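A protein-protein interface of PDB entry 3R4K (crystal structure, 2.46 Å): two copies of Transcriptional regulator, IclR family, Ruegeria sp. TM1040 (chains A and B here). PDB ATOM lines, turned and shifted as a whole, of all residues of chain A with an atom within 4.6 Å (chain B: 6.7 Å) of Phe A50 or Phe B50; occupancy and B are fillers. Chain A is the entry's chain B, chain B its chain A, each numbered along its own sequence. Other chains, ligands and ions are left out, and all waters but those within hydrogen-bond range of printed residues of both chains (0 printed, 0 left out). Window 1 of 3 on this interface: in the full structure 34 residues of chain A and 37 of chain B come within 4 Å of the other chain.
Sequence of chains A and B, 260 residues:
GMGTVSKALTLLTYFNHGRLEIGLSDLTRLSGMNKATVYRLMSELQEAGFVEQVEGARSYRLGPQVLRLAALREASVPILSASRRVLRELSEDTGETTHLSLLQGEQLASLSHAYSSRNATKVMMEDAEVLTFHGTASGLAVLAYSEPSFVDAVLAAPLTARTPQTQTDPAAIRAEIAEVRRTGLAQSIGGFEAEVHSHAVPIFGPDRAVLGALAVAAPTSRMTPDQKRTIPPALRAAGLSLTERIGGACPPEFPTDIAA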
ATOM      1  N   LEU A   9     -19.919   6.959 -10.494  1.00  0.00           N
ATOM      2  CA  LEU A   9     -19.049   6.793  -9.332  1.00  0.00           C
ATOM      3  C   LEU A   9     -18.759   5.313  -9.036  1.00  0.00           C
ATOM      4  O   LEU A   9     -17.696   5.029  -8.488  1.00  0.00           O
ATOM      5  CB  LEU A   9     -19.613   7.534  -8.105  1.00  0.00           C
ATOM      6  CG  LEU A   9     -19.813   9.048  -8.323  1.00  0.00           C
ATOM      7  CD1 LEU A   9     -20.626   9.679  -7.235  1.00  0.00           C
ATOM      8  CD2 LEU A   9     -18.515   9.772  -8.528  1.00  0.00           C
ATOM      9  N   LEU A  12     -15.459   4.083 -10.660  1.00  0.00           N
ATOM     10  CA  LEU A  12     -14.251   4.427  -9.898  1.00  0.00           C
ATOM     11  C   LEU A  12     -13.866   3.332  -8.900  1.00  0.00           C
ATOM     12  O   LEU A  12     -12.702   3.234  -8.537  1.00  0.00           O
ATOM     13  CB  LEU A  12     -14.443   5.761  -9.151  1.00  0.00           C
ATOM     14  CG  LEU A  12     -14.675   7.019  -9.994  1.00  0.00           C
ATOM     15  CD1 LEU A  12     -14.779   8.251  -9.111  1.00  0.00           C
ATOM     16  CD2 LEU A  12     -13.588   7.234 -10.992  1.00  0.00           C
ATOM     17  N   LEU A  45     -16.481  12.285 -16.153  1.00  0.00           N
ATOM     18  CA  LEU A  45     -15.568  12.248 -15.008  1.00  0.00           C
ATOM     19  C   LEU A  45     -14.228  12.881 -15.375  1.00  0.00           C
ATOM     20  O   LEU A  45     -13.621  13.553 -14.549  1.00  0.00           O
ATOM     21  CB  LEU A  45     -15.352  10.810 -14.530  1.00  0.00           C
ATOM     22  CG  LEU A  45     -16.511  10.147 -13.804  1.00  0.00           C
ATOM     23  CD1 LEU A  45     -16.352   8.631 -13.805  1.00  0.00           C
ATOM     24  CD2 LEU A  45     -16.640  10.664 -12.395  1.00  0.00           C
ATOM     25  N   ALA A  48     -14.311  16.711 -15.393  1.00  0.00           N
ATOM     26  CA  ALA A  48     -14.300  17.157 -13.999  1.00  0.00           C
ATOM     27  C   ALA A  48     -12.958  16.905 -13.284  1.00  0.00           C
ATOM     28  O   ALA A  48     -12.789  17.385 -12.177  1.00  0.00           O
ATOM     29  CB  ALA A  48     -15.420  16.474 -13.232  1.00  0.00           C
ATOM     30  N   GLY A  49     -12.033  16.180 -13.907  1.00  0.00           N
ATOM     31  CA  GLY A  49     -10.719  15.885 -13.333  1.00  0.00           C
ATOM     32  C   GLY A  49     -10.692  14.719 -12.368  1.00  0.00           C
ATOM     33  O   GLY A  49      -9.746  14.573 -11.583  1.00  0.00           O
ATOM     34  N   PHE A  50     -11.731  13.880 -12.408  1.00  0.00           N
ATOM     35  CA  PHE A  50     -11.828  12.714 -11.532  1.00  0.00           C
ATOM     36  C   PHE A  50     -11.123  11.519 -12.133  1.00  0.00           C
ATOM     37  O   PHE A  50     -10.651  10.648 -11.395  1.00  0.00           O
ATOM     38  CB  PHE A  50     -13.273  12.386 -11.211  1.00  0.00           C
ATOM     39  CG  PHE A  50     -13.805  13.216 -10.074  1.00  0.00           C
ATOM     40  CD1 PHE A  50     -14.082  14.568 -10.251  1.00  0.00           C
ATOM     41  CD2 PHE A  50     -14.026  12.650  -8.821  1.00  0.00           C
ATOM     42  CE1 PHE A  50     -14.567  15.334  -9.202  1.00  0.00           C
ATOM     43  CE2 PHE A  50     -14.481  13.429  -7.766  1.00  0.00           C
ATOM     44  CZ  PHE A  50     -14.759  14.764  -7.969  1.00  0.00           C
ATOM     45  N   VAL A  51     -11.050  11.478 -13.474  1.00  0.00           N
ATOM     46  CA  VAL A  51     -10.324  10.452 -14.227  1.00  0.00           C
ATOM     47  C   VAL A  51      -9.498  11.174 -15.283  1.00  0.00           C
ATOM     48  O   VAL A  51      -9.761  12.342 -15.591  1.00  0.00           O
ATOM     49  CB  VAL A  51     -11.185   9.294 -14.834  1.00  0.00           C
ATOM     50  CG1 VAL A  51     -12.197   8.755 -13.833  1.00  0.00           C
ATOM     51  CG2 VAL A  51     -11.860   9.694 -16.140  1.00  0.00           C
ATOM     52  N   LEU A  62      -6.968   7.375 -12.263  1.00  0.00           N
ATOM     53  CA  LEU A  62      -7.695   8.348 -11.461  1.00  0.00           C
ATOM     54  C   LEU A  62      -7.101   9.744 -11.658  1.00  0.00           C
ATOM     55  O   LEU A  62      -5.901   9.886 -11.914  1.00  0.00           O
ATOM     56  CB  LEU A  62      -7.659   7.932  -9.993  1.00  0.00           C
ATOM     57  CG  LEU A  62      -8.604   6.828  -9.617  1.00  0.00           C
ATOM     58  CD1 LEU A  62      -8.136   6.148  -8.334  1.00  0.00           C
ATOM     59  CD2 LEU A  62     -10.011   7.352  -9.507  1.00  0.00           C
ATOM     60  N   GLY A  63      -7.957  10.748 -11.584  1.00  0.00           N
ATOM     61  CA  GLY A  63      -7.584  12.147 -11.767  1.00  0.00           C
ATOM     62  C   GLY A  63      -7.231  12.864 -10.484  1.00  0.00           C
ATOM     63  O   GLY A  63      -7.464  12.324  -9.407  1.00  0.00           O
ATOM     64  N   GLN A  65      -8.593  15.399  -8.874  1.00  0.00           N
ATOM     65  CA  GLN A  65      -9.697  15.969  -8.093  1.00  0.00           C
ATOM     66  C   GLN A  65      -9.940  15.287  -6.767  1.00  0.00           C
ATOM     67  O   GLN A  65     -10.333  15.940  -5.792  1.00  0.00           O
ATOM     68  CB  GLN A  65     -11.013  15.931  -8.878  1.00  0.00           C
ATOM     69  CG  GLN A  65     -11.361  17.259  -9.495  1.00  0.00           C
ATOM     70  CD  GLN A  65     -11.401  18.364  -8.489  1.00  0.00           C
ATOM     71  OE1 GLN A  65     -12.074  18.259  -7.483  1.00  0.00           O
ATOM     72  NE2 GLN A  65     -10.610  19.398  -8.709  1.00  0.00           N
ATOM     73  N   VAL A  66      -9.727  13.972  -6.734  1.00  0.00           N
ATOM     74  CA  VAL A  66      -9.986  13.185  -5.526  1.00  0.00           C
ATOM     75  C   VAL A  66      -9.033  13.606  -4.408  1.00  0.00           C
ATOM     76  O   VAL A  66      -9.438  13.594  -3.256  1.00  0.00           O
ATOM     77  CB  VAL A  66      -9.966  11.660  -5.802  1.00  0.00           C
ATOM     78  CG1 VAL A  66     -11.122  11.277  -6.732  1.00  0.00           C
ATOM     79  CG2 VAL A  66      -8.622  11.203  -6.383  1.00  0.00           C
ATOM     80  N   LEU A  69     -10.450  16.837  -2.742  1.00  0.00           N
ATOM     81  CA  LEU A  69     -11.610  16.455  -1.940  1.00  0.00           C
ATOM     82  C   LEU A  69     -11.208  15.698  -0.674  1.00  0.00           C
ATOM     83  O   LEU A  69     -11.816  15.916   0.377  1.00  0.00           O
ATOM     84  CB  LEU A  69     -12.603  15.615  -2.752  1.00  0.00           C
ATOM     85  CG  LEU A  69     -13.186  16.242  -4.021  1.00  0.00           C
ATOM     86  CD1 LEU A  69     -14.197  15.321  -4.631  1.00  0.00           C
ATOM     87  CD2 LEU A  69     -13.809  17.591  -3.774  1.00  0.00           C
ATOM     88  N   LEU B   9     -21.007  17.082 -10.094  1.00  0.00           N
ATOM     89  CA  LEU B   9     -19.601  17.270  -9.788  1.00  0.00           C
ATOM     90  C   LEU B   9     -19.229  18.747  -9.646  1.00  0.00           C
ATOM     91  O   LEU B   9     -18.320  19.047  -8.877  1.00  0.00           O
ATOM     92  CB  LEU B   9     -18.710  16.550 -10.811  1.00  0.00           C
ATOM     93  CG  LEU B   9     -18.926  15.039 -10.875  1.00  0.00           C
ATOM     94  CD1 LEU B   9     -18.241  14.440 -12.076  1.00  0.00           C
ATOM     95  CD2 LEU B   9     -18.570  14.335  -9.529  1.00  0.00           C
ATOM     96  N   LEU B  12     -19.437  20.069  -6.001  1.00  0.00           N
ATOM     97  CA  LEU B  12     -18.278  19.745  -5.174  1.00  0.00           C
ATOM     98  C   LEU B  12     -17.196  20.824  -5.234  1.00  0.00           C
ATOM     99  O   LEU B  12     -16.428  20.954  -4.273  1.00  0.00           O
ATOM    100  CB  LEU B  12     -17.660  18.392  -5.585  1.00  0.00           C
ATOM    101  CG  LEU B  12     -18.510  17.158  -5.435  1.00  0.00           C
ATOM    102  CD1 LEU B  12     -17.747  15.953  -5.869  1.00  0.00           C
ATOM    103  CD2 LEU B  12     -18.986  16.984  -4.000  1.00  0.00           C
ATOM    104  N   GLU B  44     -27.572  11.774  -4.176  1.00  0.00           N
ATOM    105  CA  GLU B  44     -26.889  10.813  -5.019  1.00  0.00           C
ATOM    106  C   GLU B  44     -25.401  10.773  -4.663  1.00  0.00           C
ATOM    107  O   GLU B  44     -24.817   9.689  -4.638  1.00  0.00           O
ATOM    108  CB  GLU B  44     -27.095  11.158  -6.499  1.00  0.00           C
ATOM    109  CG  GLU B  44     -28.272  10.443  -7.122  1.00  0.00           C
ATOM    110  CD  GLU B  44     -28.357  10.568  -8.628  1.00  0.00           C
ATOM    111  OE1 GLU B  44     -28.955  11.566  -9.093  1.00  0.00           O
ATOM    112  OE2 GLU B  44     -27.821   9.682  -9.339  1.00  0.00           O
ATOM    113  N   LEU B  45     -24.801  11.936  -4.345  1.00  0.00           N
ATOM    114  CA  LEU B  45     -23.391  12.031  -3.940  1.00  0.00           C
ATOM    115  C   LEU B  45     -23.212  11.435  -2.541  1.00  0.00           C
ATOM    116  O   LEU B  45     -22.201  10.794  -2.273  1.00  0.00           O
ATOM    117  CB  LEU B  45     -22.895  13.473  -3.994  1.00  0.00           C
ATOM    118  CG  LEU B  45     -22.700  14.046  -5.402  1.00  0.00           C
ATOM    119  CD1 LEU B  45     -22.694  15.558  -5.376  1.00  0.00           C
ATOM    120  CD2 LEU B  45     -21.415  13.506  -6.076  1.00  0.00           C
ATOM    121  N   GLN B  46     -24.235  11.586  -1.684  1.00  0.00           N
ATOM    122  CA  GLN B  46     -24.284  11.035  -0.333  1.00  0.00           C
ATOM    123  C   GLN B  46     -24.319   9.495  -0.355  1.00  0.00           C
ATOM    124  O   GLN B  46     -23.585   8.853   0.404  1.00  0.00           O
ATOM    125  CB  GLN B  46     -25.496  11.592   0.406  1.00  0.00           C
ATOM    126  CG  GLN B  46     -25.410  11.518   1.912  1.00  0.00           C
ATOM    127  CD  GLN B  46     -26.659  12.037   2.584  1.00  0.00           C
ATOM    128  OE1 GLN B  46     -27.515  12.709   1.977  1.00  0.00           O
ATOM    129  NE2 GLN B  46     -26.777  11.741   3.871  1.00  0.00           N
ATOM    130  N   GLU B  47     -25.148   8.908  -1.233  1.00  0.00           N
ATOM    131  CA  GLU B  47     -25.240   7.450  -1.363  1.00  0.00           C
ATOM    132  C   GLU B  47     -23.890   6.839  -1.825  1.00  0.00           C
ATOM    133  O   GLU B  47     -23.559   5.718  -1.444  1.00  0.00           O
ATOM    134  CB  GLU B  47     -26.370   7.060  -2.320  1.00  0.00           C
ATOM    135  CG  GLU B  47     -26.997   5.718  -1.942  1.00  0.00           C
ATOM    136  CD  GLU B  47     -27.921   5.631  -0.728  1.00  0.00           C
ATOM    137  OE1 GLU B  47     -28.347   6.688  -0.203  1.00  0.00           O
ATOM    138  OE2 GLU B  47     -28.234   4.490  -0.311  1.00  0.00           O
ATOM    139  N   ALA B  48     -23.107   7.602  -2.602  1.00  0.00           N
ATOM    140  CA  ALA B  48     -21.789   7.197  -3.098  1.00  0.00           C
ATOM    141  C   ALA B  48     -20.667   7.468  -2.088  1.00  0.00           C
ATOM    142  O   ALA B  48     -19.544   7.036  -2.310  1.00  0.00           O
ATOM    143  CB  ALA B  48     -21.481   7.902  -4.405  1.00  0.00           C
ATOM    144  N   GLY B  49     -20.977   8.161  -1.001  1.00  0.00           N
ATOM    145  CA  GLY B  49     -20.017   8.490   0.046  1.00  0.00           C
ATOM    146  C   GLY B  49     -19.151   9.698  -0.248  1.00  0.00           C
ATOM    147  O   GLY B  49     -18.147   9.902   0.433  1.00  0.00           O
ATOM    148  N   PHE B  50     -19.526  10.510  -1.249  1.00  0.00           N
ATOM    149  CA  PHE B  50     -18.783  11.698  -1.646  1.00  0.00           C
ATOM    150  C   PHE B  50     -19.168  12.885  -0.799  1.00  0.00           C
ATOM    151  O   PHE B  50     -18.332  13.754  -0.610  1.00  0.00           O
ATOM    152  CB  PHE B  50     -19.000  11.987  -3.133  1.00  0.00           C
ATOM    153  CG  PHE B  50     -18.047  11.187  -3.993  1.00  0.00           C
ATOM    154  CD1 PHE B  50     -18.132   9.793  -4.055  1.00  0.00           C
ATOM    155  CD2 PHE B  50     -17.077  11.821  -4.764  1.00  0.00           C
ATOM    156  CE1 PHE B  50     -17.235   9.051  -4.830  1.00  0.00           C
ATOM    157  CE2 PHE B  50     -16.215  11.080  -5.588  1.00  0.00           C
ATOM    158  CZ  PHE B  50     -16.279   9.702  -5.591  1.00  0.00           C
ATOM    159  N   VAL B  51     -20.427  12.961  -0.331  1.00  0.00           N
ATOM    160  CA  VAL B  51     -20.874  14.028   0.558  1.00  0.00           C
ATOM    161  C   VAL B  51     -21.622  13.393   1.746  1.00  0.00           C
ATOM    162  O   VAL B  51     -22.034  12.231   1.679  1.00  0.00           O
ATOM    163  CB  VAL B  51     -21.706  15.168  -0.122  1.00  0.00           C
ATOM    164  CG1 VAL B  51     -21.099  15.623  -1.436  1.00  0.00           C
ATOM    165  CG2 VAL B  51     -23.179  14.805  -0.296  1.00  0.00           C
ATOM    166  N   GLU B  52     -21.773  14.144   2.842  1.00  0.00           N
ATOM    167  CA  GLU B  52     -22.568  13.679   3.975  1.00  0.00           C
ATOM    168  C   GLU B  52     -23.271  14.862   4.636  1.00  0.00           C
ATOM    169  O   GLU B  52     -22.804  15.998   4.530  1.00  0.00           O
ATOM    170  CB  GLU B  52     -21.764  12.835   4.981  1.00  0.00           C
ATOM    171  CG  GLU B  52     -20.658  13.531   5.742  1.00  0.00           C
ATOM    172  CD  GLU B  52     -19.992  12.640   6.770  1.00  0.00           C
ATOM    173  OE1 GLU B  52     -19.955  11.404   6.572  1.00  0.00           O
ATOM    174  OE2 GLU B  52     -19.490  13.186   7.776  1.00  0.00           O
ATOM    175  N   ARG B  61     -21.147  18.395   4.029  1.00  0.00           N
ATOM    176  CA  ARG B  61     -19.694  18.410   4.047  1.00  0.00           C
ATOM    177  C   ARG B  61     -19.234  17.236   3.196  1.00  0.00           C
ATOM    178  O   ARG B  61     -20.046  16.357   2.866  1.00  0.00           O
ATOM    179  CB  ARG B  61     -19.118  18.379   5.464  1.00  0.00           C
ATOM    180  CG  ARG B  61     -19.359  17.090   6.213  1.00  0.00           C
ATOM    181  CD  ARG B  61     -18.750  17.180   7.577  1.00  0.00           C
ATOM    182  NE  ARG B  61     -18.699  15.869   8.216  1.00  0.00           N
ATOM    183  CZ  ARG B  61     -18.359  15.672   9.485  1.00  0.00           C
ATOM    184  NH1 ARG B  61     -18.062  16.704  10.269  1.00  0.00           N
ATOM    185  NH2 ARG B  61     -18.329  14.442   9.987  1.00  0.00           N
ATOM    186  N   LEU B  62     -17.956  17.223   2.822  1.00  0.00           N
ATOM    187  CA  LEU B  62     -17.419  16.147   2.006  1.00  0.00           C
ATOM    188  C   LEU B  62     -17.415  14.812   2.772  1.00  0.00           C
ATOM    189  O   LEU B  62     -17.318  14.791   3.998  1.00  0.00           O
ATOM    190  CB  LEU B  62     -16.039  16.501   1.448  1.00  0.00           C
ATOM    191  CG  LEU B  62     -16.105  17.538   0.313  1.00  0.00           C
ATOM    192  CD1 LEU B  62     -14.819  18.146   0.102  1.00  0.00           C
ATOM    193  CD2 LEU B  62     -16.553  16.915  -1.013  1.00  0.00           C
ATOM    194  N   GLY B  63     -17.662  13.739   2.029  1.00  0.00           N
ATOM    195  CA  GLY B  63     -17.783  12.370   2.522  1.00  0.00           C
ATOM    196  C   GLY B  63     -16.490  11.568   2.602  1.00  0.00           C
ATOM    197  O   GLY B  63     -15.453  11.959   2.060  1.00  0.00           O
ATOM    198  N   PRO B  64     -16.534  10.387   3.246  1.00  0.00           N
ATOM    199  CA  PRO B  64     -15.282   9.616   3.456  1.00  0.00           C
ATOM    200  C   PRO B  64     -14.781   8.770   2.299  1.00  0.00           C
ATOM    201  O   PRO B  64     -13.626   8.353   2.331  1.00  0.00           O
ATOM    202  CB  PRO B  64     -15.644   8.693   4.616  1.00  0.00           C
ATOM    203  CG  PRO B  64     -17.132   8.491   4.486  1.00  0.00           C
ATOM    204  CD  PRO B  64     -17.681   9.783   3.966  1.00  0.00           C
ATOM    205  N   GLN B  65     -15.627   8.467   1.308  1.00  0.00           N
ATOM    206  CA  GLN B  65     -15.227   7.578   0.195  1.00  0.00           C
ATOM    207  C   GLN B  65     -14.177   8.150  -0.801  1.00  0.00           C
ATOM    208  O   GLN B  65     -13.623   7.374  -1.578  1.00  0.00           O
ATOM    209  CB  GLN B  65     -16.445   7.024  -0.546  1.00  0.00           C
ATOM    210  CG  GLN B  65     -17.150   5.995   0.354  1.00  0.00           C
ATOM    211  CD  GLN B  65     -17.924   4.942  -0.364  1.00  0.00           C
ATOM    212  OE1 GLN B  65     -19.124   4.783  -0.117  1.00  0.00           O
ATOM    213  NE2 GLN B  65     -17.248   4.140  -1.197  1.00  0.00           N
ATOM    214  N   VAL B  66     -13.813   9.429  -0.699  1.00  0.00           N
ATOM    215  CA  VAL B  66     -12.778  10.074  -1.501  1.00  0.00           C
ATOM    216  C   VAL B  66     -11.400   9.692  -0.974  1.00  0.00           C
ATOM    217  O   VAL B  66     -10.413   9.806  -1.709  1.00  0.00           O
ATOM    218  CB  VAL B  66     -12.937  11.630  -1.576  1.00  0.00           C
ATOM    219  CG1 VAL B  66     -14.188  12.023  -2.352  1.00  0.00           C
ATOM    220  CG2 VAL B  66     -12.934  12.288  -0.196  1.00  0.00           C
ATOM    221  N   LEU B  69      -9.814   6.675  -2.891  1.00  0.00           N
ATOM    222  CA  LEU B  69      -9.513   7.119  -4.255  1.00  0.00           C
ATOM    223  C   LEU B  69      -8.295   8.025  -4.292  1.00  0.00           C
ATOM    224  O   LEU B  69      -7.495   7.906  -5.215  1.00  0.00           O
ATOM    225  CB  LEU B  69     -10.729   7.830  -4.886  1.00  0.00           C
ATOM    226  CG  LEU B  69     -12.014   7.004  -5.014  1.00  0.00           C
ATOM    227  CD1 LEU B  69     -13.136   7.833  -5.626  1.00  0.00           C
ATOM    228  CD2 LEU B  69     -11.772   5.684  -5.780  1.00  0.00           C
ATOM    229  N   ARG B  73      -4.823   7.436  -6.318  1.00  0.00           N
ATOM    230  CA  ARG B  73      -4.331   8.509  -7.192  1.00  0.00           C
ATOM    231  C   ARG B  73      -2.850   8.814  -6.878  1.00  0.00           C
ATOM    232  O   ARG B  73      -2.026   8.928  -7.804  1.00  0.00           O
ATOM    233  CB  ARG B  73      -5.201   9.765  -7.085  1.00  0.00           C
ATOM    234  CG  ARG B  73      -4.582  11.017  -7.734  1.00  0.00           C
ATOM    235  CD  ARG B  73      -4.417  10.964  -9.239  1.00  0.00           C
ATOM    236  NE  ARG B  73      -3.681  12.139  -9.687  1.00  0.00           N
ATOM    237  CZ  ARG B  73      -3.464  12.475 -10.949  1.00  0.00           C
ATOM    238  NH1 ARG B  73      -3.890  11.694 -11.935  1.00  0.00           N
ATOM    239  NH2 ARG B  73      -2.769  13.563 -11.237  1.00  0.00           N
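The backbone carbonyl oxygen of Leu A62 is in hydrogen-bond range of the guanidinium group of Arg B73, 2.7 Å away.
The backbone carbonyl oxygen (O) of Leu B45 lies within hydrogen-bond range of the backbone NH (N) of Phe B50 (2.9 Å). OE1 of Gln B65 lies close to O of Ala B48, at 3.2 Å. The backbone carbonyl oxygen of Phe B50 sits at hydrogen-bond distance from the backbone NH of Gly B63 (2.7 Å). The backbone carbonyl oxygen (O) of Leu A45 is in hydrogen-bond range of the backbone NH (N) of Phe A50. O of Phe A50 sits at hydrogen-bond distance from N of Gly A63 (2.7 Å).
Printed residues of chain B within 4 Å of Ala A48: Leu B9 (3.7 Å). Of chain B, only Leu B12 (3.8 Å) and Phe B50 (3.6 Å) come within 4 Å of Phe A50. Of the printed residues of chain B, Leu A62 touches Leu B69 (3.6 Å) and Arg B73 (2.7 Å). Of the printed residues of chain B, Leu A69 touches Leu B12 (3.8 Å), Leu B62 (3.8 Å) and Val B66 (3.8 Å). Of the printed residues of chain A, Leu B12 touches Phe A50 (3.8 Å) and Leu A69 (3.8 Å). Of the printed residues of chain A, Ala B48 touches Leu A9 (3.4 Å). Of the printed residues of chain A, Phe B50 touches Leu A9 (3.7 Å) and Phe A50 (3.6 Å). The nearest residue of chain B that does not touch Phe A50 is Leu B9 (4.1 Å). The nearest residue of chain A that does not touch Phe B50 is Leu A12 (4.1 Å).
Leu A9 touches Ala B48. CD2 of Leu A9 touches CZ of Phe B50 (3.7 Å). Ala A48 touches Leu B9 (CB to CD1, 3.7 Å). Leu B12 touches Phe A50. Phe A50 touches Phe B50. CD1 of Leu A62 touches O of Leu B69 (3.6 Å). Arg B73 touches Gly A63. Val A66 touches Leu B69 (CG2 to O, 3.7 Å). CD1 of Leu A69 touches CD1 of Leu B12 (3.8 Å). Leu A69 touches Val B66 (O to CG2, 3.8 Å).
Leu A9 touches Phe B50, but with the chains exchanged Phe A50 does not touch Leu B9 (4.1 Å). Phe A50 touches Leu B12, but with the chains exchanged Leu A12 does not touch Phe B50 (4.1 Å). Phe A50 touches its own counterpart, Phe B50. Val A66 touches Leu B69, and with the chains exchanged Leu A69 touches Val B66. 12 positions are printed for both chains.
Hydrophobic or aromatic side chains of chain A within 4 Å of the printed part of chain B: Leu A9, Leu A12, Ala A48, Phe A50, Leu A62, Val A66 and Leu A69. Among the printed residues, no Asp or Glu carboxylate lies within 4 Å of a Lys or Arg side-chain nitrogen of the other chain.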
